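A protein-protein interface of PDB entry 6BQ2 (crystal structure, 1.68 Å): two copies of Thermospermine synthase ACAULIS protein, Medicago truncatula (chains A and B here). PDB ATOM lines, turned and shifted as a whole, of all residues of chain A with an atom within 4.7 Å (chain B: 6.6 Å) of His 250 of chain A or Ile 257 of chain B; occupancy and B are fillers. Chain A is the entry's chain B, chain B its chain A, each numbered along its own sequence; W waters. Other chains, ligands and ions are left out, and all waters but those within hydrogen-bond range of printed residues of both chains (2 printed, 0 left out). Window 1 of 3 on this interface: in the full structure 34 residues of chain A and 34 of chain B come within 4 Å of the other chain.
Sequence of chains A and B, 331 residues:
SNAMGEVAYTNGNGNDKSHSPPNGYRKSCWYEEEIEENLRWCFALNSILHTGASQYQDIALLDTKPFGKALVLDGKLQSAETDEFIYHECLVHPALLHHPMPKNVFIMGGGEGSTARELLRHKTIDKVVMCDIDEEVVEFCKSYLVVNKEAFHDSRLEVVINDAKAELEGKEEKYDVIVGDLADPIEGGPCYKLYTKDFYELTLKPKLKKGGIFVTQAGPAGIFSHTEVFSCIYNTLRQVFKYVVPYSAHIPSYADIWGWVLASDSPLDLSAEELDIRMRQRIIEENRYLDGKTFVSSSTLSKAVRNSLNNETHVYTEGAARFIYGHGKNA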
ATOM      1  N   ILE A  86     -32.633  18.103  17.508  1.00  0.00           N
ATOM      2  CA  ILE A  86     -32.270  17.896  18.893  1.00  0.00           C
ATOM      3  C   ILE A  86     -31.727  19.200  19.468  1.00  0.00           C
ATOM      4  O   ILE A  86     -32.162  19.649  20.540  1.00  0.00           O
ATOM      5  CB  ILE A  86     -31.237  16.763  19.067  1.00  0.00           C
ATOM      6  CG1 ILE A  86     -31.773  15.461  18.459  1.00  0.00           C
ATOM      7  CG2 ILE A  86     -30.829  16.566  20.553  1.00  0.00           C
ATOM      8  CD1 ILE A  86     -30.778  14.331  18.505  1.00  0.00           C
ATOM      9  N   SER A 248     -27.976  19.122  29.233  1.00  0.00           N
ATOM     10  CA  SER A 248     -27.187  18.650  28.104  1.00  0.00           C
ATOM     11  C   SER A 248     -27.841  17.495  27.369  1.00  0.00           C
ATOM     12  O   SER A 248     -28.763  16.863  27.916  1.00  0.00           O
ATOM     13  CB  SER A 248     -25.790  18.292  28.631  1.00  0.00           C
ATOM     14  OG  SER A 248     -25.882  17.125  29.451  1.00  0.00           O
ATOM     15  N   ALA A 249     -27.387  17.189  26.146  1.00  0.00           N
ATOM     16  CA  ALA A 249     -27.967  16.096  25.352  1.00  0.00           C
ATOM     17  C   ALA A 249     -27.021  15.771  24.258  1.00  0.00           C
ATOM     18  O   ALA A 249     -26.295  16.641  23.785  1.00  0.00           O
ATOM     19  CB  ALA A 249     -29.289  16.524  24.753  1.00  0.00           C
ATOM     20  N   HIS A 250     -26.976  14.500  23.887  1.00  0.00           N
ATOM     21  CA  HIS A 250     -26.081  14.080  22.819  1.00  0.00           C
ATOM     22  C   HIS A 250     -26.584  14.534  21.467  1.00  0.00           C
ATOM     23  O   HIS A 250     -27.768  14.380  21.171  1.00  0.00           O
ATOM     24  CB  HIS A 250     -26.020  12.538  22.830  1.00  0.00           C
ATOM     25  CG  HIS A 250     -25.082  11.930  21.833  1.00  0.00           C
ATOM     26  ND1 HIS A 250     -25.527  11.108  20.825  1.00  0.00           N
ATOM     27  CD2 HIS A 250     -23.746  12.018  21.679  1.00  0.00           C
ATOM     28  CE1 HIS A 250     -24.509  10.726  20.082  1.00  0.00           C
ATOM     29  NE2 HIS A 250     -23.413  11.285  20.570  1.00  0.00           N
ATOM     30  N   ILE A 251     -25.673  15.030  20.633  1.00  0.00           N
ATOM     31  CA  ILE A 251     -25.995  15.342  19.223  1.00  0.00           C
ATOM     32  C   ILE A 251     -25.025  14.556  18.311  1.00  0.00           C
ATOM     33  O   ILE A 251     -23.845  14.842  18.271  1.00  0.00           O
ATOM     34  CB  ILE A 251     -25.951  16.853  18.974  1.00  0.00           C
ATOM     35  CG1 ILE A 251     -26.976  17.517  19.921  1.00  0.00           C
ATOM     36  CG2 ILE A 251     -26.350  17.169  17.536  1.00  0.00           C
ATOM     37  CD1 ILE A 251     -26.965  18.995  19.991  1.00  0.00           C
ATOM     38  N   PRO A 252     -25.514  13.531  17.614  1.00  0.00           N
ATOM     39  CA  PRO A 252     -24.603  12.643  16.911  1.00  0.00           C
ATOM     40  C   PRO A 252     -23.668  13.372  15.950  1.00  0.00           C
ATOM     41  O   PRO A 252     -22.472  13.108  15.961  1.00  0.00           O
ATOM     42  CB  PRO A 252     -25.535  11.679  16.169  1.00  0.00           C
ATOM     43  CG  PRO A 252     -26.756  11.645  16.999  1.00  0.00           C
ATOM     44  CD  PRO A 252     -26.873  12.961  17.706  1.00  0.00           C
ATOM     45  N   ASP A 256     -20.450  14.710  20.261  1.00  0.00           N
ATOM     46  CA  ASP A 256     -20.291  14.976  21.674  1.00  0.00           C
ATOM     47  C   ASP A 256     -21.662  15.261  22.271  1.00  0.00           C
ATOM     48  O   ASP A 256     -22.660  15.445  21.542  1.00  0.00           O
ATOM     49  CB  ASP A 256     -19.357  16.171  21.933  1.00  0.00           C
ATOM     50  CG  ASP A 256     -18.670  16.138  23.328  1.00  0.00           C
ATOM     51  OD1 ASP A 256     -18.977  15.274  24.205  1.00  0.00           O
ATOM     52  OD2 ASP A 256     -17.805  17.006  23.539  1.00  0.00           O
ATOM     53  N   ILE A 257     -21.678  15.273  23.590  1.00  0.00           N
ATOM     54  CA  ILE A 257     -22.746  15.816  24.381  1.00  0.00           C
ATOM     55  C   ILE A 257     -22.621  17.352  24.209  1.00  0.00           C
ATOM     56  O   ILE A 257     -21.529  17.890  24.247  1.00  0.00           O
ATOM     57  CB  ILE A 257     -22.624  15.426  25.859  1.00  0.00           C
ATOM     58  CG1 ILE A 257     -22.594  13.887  25.991  1.00  0.00           C
ATOM     59  CG2 ILE A 257     -23.725  16.037  26.672  1.00  0.00           C
ATOM     60  CD1 ILE A 257     -23.830  13.211  25.452  1.00  0.00           C
ATOM     61  N   GLY B 219     -24.927  -2.486  23.452  1.00  0.00           N
ATOM     62  CA  GLY B 219     -24.530  -1.850  22.198  1.00  0.00           C
ATOM     63  C   GLY B 219     -24.806  -0.362  22.188  1.00  0.00           C
ATOM     64  O   GLY B 219     -25.187   0.219  23.229  1.00  0.00           O
ATOM     65  N   PRO B 220     -24.686   0.257  21.015  1.00  0.00           N
ATOM     66  CA  PRO B 220     -24.963   1.714  20.900  1.00  0.00           C
ATOM     67  C   PRO B 220     -26.394   2.040  21.296  1.00  0.00           C
ATOM     68  O   PRO B 220     -27.334   1.249  21.065  1.00  0.00           O
ATOM     69  CB  PRO B 220     -24.724   1.988  19.426  1.00  0.00           C
ATOM     70  CG  PRO B 220     -23.788   0.914  18.970  1.00  0.00           C
ATOM     71  CD  PRO B 220     -24.236  -0.292  19.730  1.00  0.00           C
ATOM     72  N   ALA B 221     -26.592   3.182  21.912  1.00  0.00           N
ATOM     73  CA  ALA B 221     -27.903   3.618  22.417  1.00  0.00           C
ATOM     74  C   ALA B 221     -28.196   5.092  22.044  1.00  0.00           C
ATOM     75  O   ALA B 221     -28.873   5.817  22.763  1.00  0.00           O
ATOM     76  CB  ALA B 221     -28.027   3.351  23.898  1.00  0.00           C
ATOM     77  N   GLY B 222     -27.672   5.487  20.876  1.00  0.00           N
ATOM     78  CA  GLY B 222     -27.854   6.831  20.307  1.00  0.00           C
ATOM     79  C   GLY B 222     -29.271   6.980  19.781  1.00  0.00           C
ATOM     80  O   GLY B 222     -30.005   5.995  19.622  1.00  0.00           O
ATOM     81  N   ILE B 223     -29.648   8.218  19.527  1.00  0.00           N
ATOM     82  CA  ILE B 223     -30.999   8.557  19.078  1.00  0.00           C
ATOM     83  C   ILE B 223     -31.422   7.721  17.866  1.00  0.00           C
ATOM     84  O   ILE B 223     -32.558   7.300  17.819  1.00  0.00           O
ATOM     85  CB  ILE B 223     -31.139  10.058  18.845  1.00  0.00           C
ATOM     86  CG1 ILE B 223     -32.528  10.439  18.291  1.00  0.00           C
ATOM     87  CG2 ILE B 223     -30.103  10.594  17.872  1.00  0.00           C
ATOM     88  CD1 ILE B 223     -33.552  10.424  19.346  1.00  0.00           C
ATOM     89  N   SER B 225     -28.826   5.177  16.537  1.00  0.00           N
ATOM     90  CA  SER B 225     -28.000   3.975  16.596  1.00  0.00           C
ATOM     91  C   SER B 225     -28.576   2.922  17.484  1.00  0.00           C
ATOM     92  O   SER B 225     -28.215   1.729  17.334  1.00  0.00           O
ATOM     93  CB  SER B 225     -26.579   4.296  17.035  1.00  0.00           C
ATOM     94  OG  SER B 225     -26.529   4.833  18.337  1.00  0.00           O
ATOM     95  N   SER B 248     -28.460   4.203  29.811  1.00  0.00           N
ATOM     96  CA  SER B 248     -27.411   4.532  28.866  1.00  0.00           C
ATOM     97  C   SER B 248     -26.534   5.665  29.328  1.00  0.00           C
ATOM     98  O   SER B 248     -26.915   6.414  30.212  1.00  0.00           O
ATOM     99  CB  SER B 248     -28.015   4.851  27.496  1.00  0.00           C
ATOM    100  OG  SER B 248     -28.855   6.041  27.514  1.00  0.00           O
ATOM    101  N   ALA B 249     -25.362   5.806  28.716  1.00  0.00           N
ATOM    102  CA  ALA B 249     -24.437   6.882  29.049  1.00  0.00           C
ATOM    103  C   ALA B 249     -23.440   7.089  27.926  1.00  0.00           C
ATOM    104  O   ALA B 249     -23.077   6.161  27.239  1.00  0.00           O
ATOM    105  CB  ALA B 249     -23.666   6.557  30.312  1.00  0.00           C
ATOM    106  N   HIS B 250     -23.031   8.334  27.736  1.00  0.00           N
ATOM    107  CA  HIS B 250     -21.989   8.658  26.748  1.00  0.00           C
ATOM    108  C   HIS B 250     -20.617   8.101  27.117  1.00  0.00           C
ATOM    109  O   HIS B 250     -20.165   8.288  28.225  1.00  0.00           O
ATOM    110  CB  HIS B 250     -21.885  10.174  26.604  1.00  0.00           C
ATOM    111  CG  HIS B 250     -21.010  10.625  25.476  1.00  0.00           C
ATOM    112  ND1 HIS B 250     -19.943  11.462  25.650  1.00  0.00           N
ATOM    113  CD2 HIS B 250     -21.040  10.339  24.155  1.00  0.00           C
ATOM    114  CE1 HIS B 250     -19.352  11.684  24.492  1.00  0.00           C
ATOM    115  NE2 HIS B 250     -19.984  10.984  23.570  1.00  0.00           N
ATOM    116  N   ILE B 251     -19.959   7.436  26.177  1.00  0.00           N
ATOM    117  CA  ILE B 251     -18.561   7.037  26.353  1.00  0.00           C
ATOM    118  C   ILE B 251     -17.805   7.677  25.190  1.00  0.00           C
ATOM    119  O   ILE B 251     -17.931   7.209  24.069  1.00  0.00           O
ATOM    120  CB  ILE B 251     -18.388   5.524  26.371  1.00  0.00           C
ATOM    121  CG1 ILE B 251     -19.268   4.923  27.491  1.00  0.00           C
ATOM    122  CG2 ILE B 251     -16.924   5.182  26.642  1.00  0.00           C
ATOM    123  CD1 ILE B 251     -19.548   3.481  27.314  1.00  0.00           C
ATOM    124  N   TYR B 254     -16.070   5.538  22.501  1.00  0.00           N
ATOM    125  CA  TYR B 254     -16.978   4.668  21.731  1.00  0.00           C
ATOM    126  C   TYR B 254     -17.704   5.445  20.647  1.00  0.00           C
ATOM    127  O   TYR B 254     -18.443   4.839  19.850  1.00  0.00           O
ATOM    128  CB  TYR B 254     -18.022   4.027  22.637  1.00  0.00           C
ATOM    129  CG  TYR B 254     -17.564   2.909  23.593  1.00  0.00           C
ATOM    130  CD1 TYR B 254     -16.356   2.953  24.266  1.00  0.00           C
ATOM    131  CD2 TYR B 254     -18.375   1.847  23.846  1.00  0.00           C
ATOM    132  CE1 TYR B 254     -15.975   1.918  25.136  1.00  0.00           C
ATOM    133  CE2 TYR B 254     -18.005   0.812  24.701  1.00  0.00           C
ATOM    134  CZ  TYR B 254     -16.808   0.859  25.353  1.00  0.00           C
ATOM    135  OH  TYR B 254     -16.438  -0.197  26.203  1.00  0.00           O
ATOM    136  N   ALA B 255     -17.560   6.770  20.631  1.00  0.00           N
ATOM    137  CA  ALA B 255     -18.166   7.620  19.651  1.00  0.00           C
ATOM    138  C   ALA B 255     -19.701   7.617  19.677  1.00  0.00           C
ATOM    139  O   ALA B 255     -20.336   8.000  18.686  1.00  0.00           O
ATOM    140  CB  ALA B 255     -17.636   7.272  18.235  1.00  0.00           C
ATOM    141  N   ASP B 256     -20.296   7.265  20.828  1.00  0.00           N
ATOM    142  CA  ASP B 256     -21.726   7.167  20.912  1.00  0.00           C
ATOM    143  C   ASP B 256     -22.124   7.092  22.376  1.00  0.00           C
ATOM    144  O   ASP B 256     -21.272   6.874  23.252  1.00  0.00           O
ATOM    145  CB  ASP B 256     -22.218   5.902  20.182  1.00  0.00           C
ATOM    146  CG  ASP B 256     -23.618   6.067  19.569  1.00  0.00           C
ATOM    147  OD1 ASP B 256     -24.334   7.012  19.980  1.00  0.00           O
ATOM    148  OD2 ASP B 256     -23.997   5.241  18.707  1.00  0.00           O
ATOM    149  N   ILE B 257     -23.418   7.208  22.582  1.00  0.00           N
ATOM    150  CA  ILE B 257     -24.099   6.780  23.798  1.00  0.00           C
ATOM    151  C   ILE B 257     -24.059   5.236  23.744  1.00  0.00           C
ATOM    152  O   ILE B 257     -24.291   4.625  22.674  1.00  0.00           O
ATOM    153  CB  ILE B 257     -25.563   7.270  23.803  1.00  0.00           C
ATOM    154  CG1 ILE B 257     -25.642   8.774  23.681  1.00  0.00           C
ATOM    155  CG2 ILE B 257     -26.291   6.774  25.029  1.00  0.00           C
ATOM    156  CD1 ILE B 257     -24.799   9.481  24.727  1.00  0.00           C
ATOM    157  N   TRP B 258     -23.760   4.646  24.893  1.00  0.00           N
ATOM    158  CA  TRP B 258     -23.781   3.209  25.040  1.00  0.00           C
ATOM    159  C   TRP B 258     -24.913   2.816  25.962  1.00  0.00           C
ATOM    160  O   TRP B 258     -25.287   3.548  26.848  1.00  0.00           O
ATOM    161  CB  TRP B 258     -22.434   2.714  25.544  1.00  0.00           C
ATOM    162  CG  TRP B 258     -22.113   1.382  25.027  1.00  0.00           C
ATOM    163  CD1 TRP B 258     -22.184   0.174  25.684  1.00  0.00           C
ATOM    164  CD2 TRP B 258     -21.721   1.101  23.699  1.00  0.00           C
ATOM    165  NE1 TRP B 258     -21.833  -0.845  24.827  1.00  0.00           N
ATOM    166  CE2 TRP B 258     -21.565  -0.306  23.592  1.00  0.00           C
ATOM    167  CE3 TRP B 258     -21.505   1.888  22.584  1.00  0.00           C
ATOM    168  CZ2 TRP B 258     -21.154  -0.908  22.405  1.00  0.00           C
ATOM    169  CZ3 TRP B 258     -21.109   1.297  21.405  1.00  0.00           C
ATOM    170  CH2 TRP B 258     -20.929  -0.090  21.328  1.00  0.00           C
ATOM    171  N   GLY B 259     -25.396   1.596  25.780  1.00  0.00           N
ATOM    172  CA  GLY B 259     -26.469   1.068  26.544  1.00  0.00           C
ATOM    173  C   GLY B 259     -26.188  -0.201  27.329  1.00  0.00           C
ATOM    174  O   GLY B 259     -25.289  -0.976  26.989  1.00  0.00           O
HETATM  175  O   HOH W   1     -21.149  10.816  18.929  1.00  0.00           O
HETATM  176  O   HOH W   2     -28.140  10.230  20.947  1.00  0.00           O
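Of the 16 printed residues of chain B, 4 touch a printed residue of chain A. Hydrophobic or aromatic side chains of chain B within 4 Å of the printed part of chain A: Ile 223, His 250 and Ile 257. Printed residues of chain A that touch a printed residue of chain B: Ile 86, His 250, Pro 252, Asp 256 and Ile 257. Hydrophobic or aromatic side chains of chain A within 4 Å of the printed part of chain B: Ile 86, His 250, Pro 252 and Ile 257. Along chain A the printed residues that touch a printed residue of chain B span positions 86 to 257. Among the printed residues, no Asp or Glu carboxylate lies within 4 Å of a Lys or Arg side-chain nitrogen of the other chain.
Among the printed residues, merely in contact across the chains: Ile 257 of chain A with His 250 of chain B (3.6 Å), Pro 252 of chain A with Ile 223 of chain B (3.6 Å), Asp 256 of chain A with His 250 of chain B (3.6 Å), His 250 of chain A with Ile 257 of chain B (3.7 Å), His 250 of chain A with Asp 256 of chain B (3.7 Å), Ile 86 of chain A with Ile 223 of chain B (3.8 Å) and Ile 257 of chain A with Ile 257 of chain B (3.9 Å).
Water W2 lies within hydrogen-bond range of ND1 of His 250 of chain A (2.8 Å) and N of Ile 223 of chain B (2.9 Å). Water W1 lies within hydrogen-bond range of a ring nitrogen (NE2) of His 250 of chain A (2.8 Å) and the backbone carbonyl oxygen (O) of Ala 255 of chain B (2.9 Å).
Printed residues of chain B within 4 Å of Ile 86 of chain A: Ile 223. Ala 249 of chain A touches none of the printed residues of chain B. His 250 of chain A touches just these residues of chain B: Asp 256 and Ile 257. Printed residues of chain A within 4 Å of His 250 of chain B: Asp 256 and Ile 257. Of chain A, only His 250 (3.7 Å) and Ile 257 (3.9 Å) come within 4 Å of Ile 257 of chain B. The nearest printed residue of chain B that does not touch Ile 257 of chain A is Ala 249 of chain B (6.6 Å).
His 250 of chain A touches Asp 256 of chain B, and with the chains exchanged Asp 256 of chain A touches His 250 of chain B. His 250 of chain A touches Ile 257 of chain B, and with the chains exchanged Ile 257 of chain A touches His 250 of chain B. Ile 257 of chain A touches its own counterpart, Ile 257 of chain B. 6 positions are printed for both chains.
The backbone carbonyl oxygen (O) of Asp 256 of chain B is in hydrogen-bond range of the backbone NH (N) of Ile 251 of chain B (3.3 Å). The backbone carbonyl oxygen of Ile 257 of chain B lies within hydrogen-bond range of the backbone NH of Ala 221 of chain B, 2.8 Å away. The side-chain carboxylate of Asp 256 of chain B lies within hydrogen-bond range of the side-chain hydroxyl of Ser 225 of chain B, 2.6 Å away. N of Ile 251 of chain A lies within hydrogen-bond range of O of Asp 256 of chain A, at 3.2 Å.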
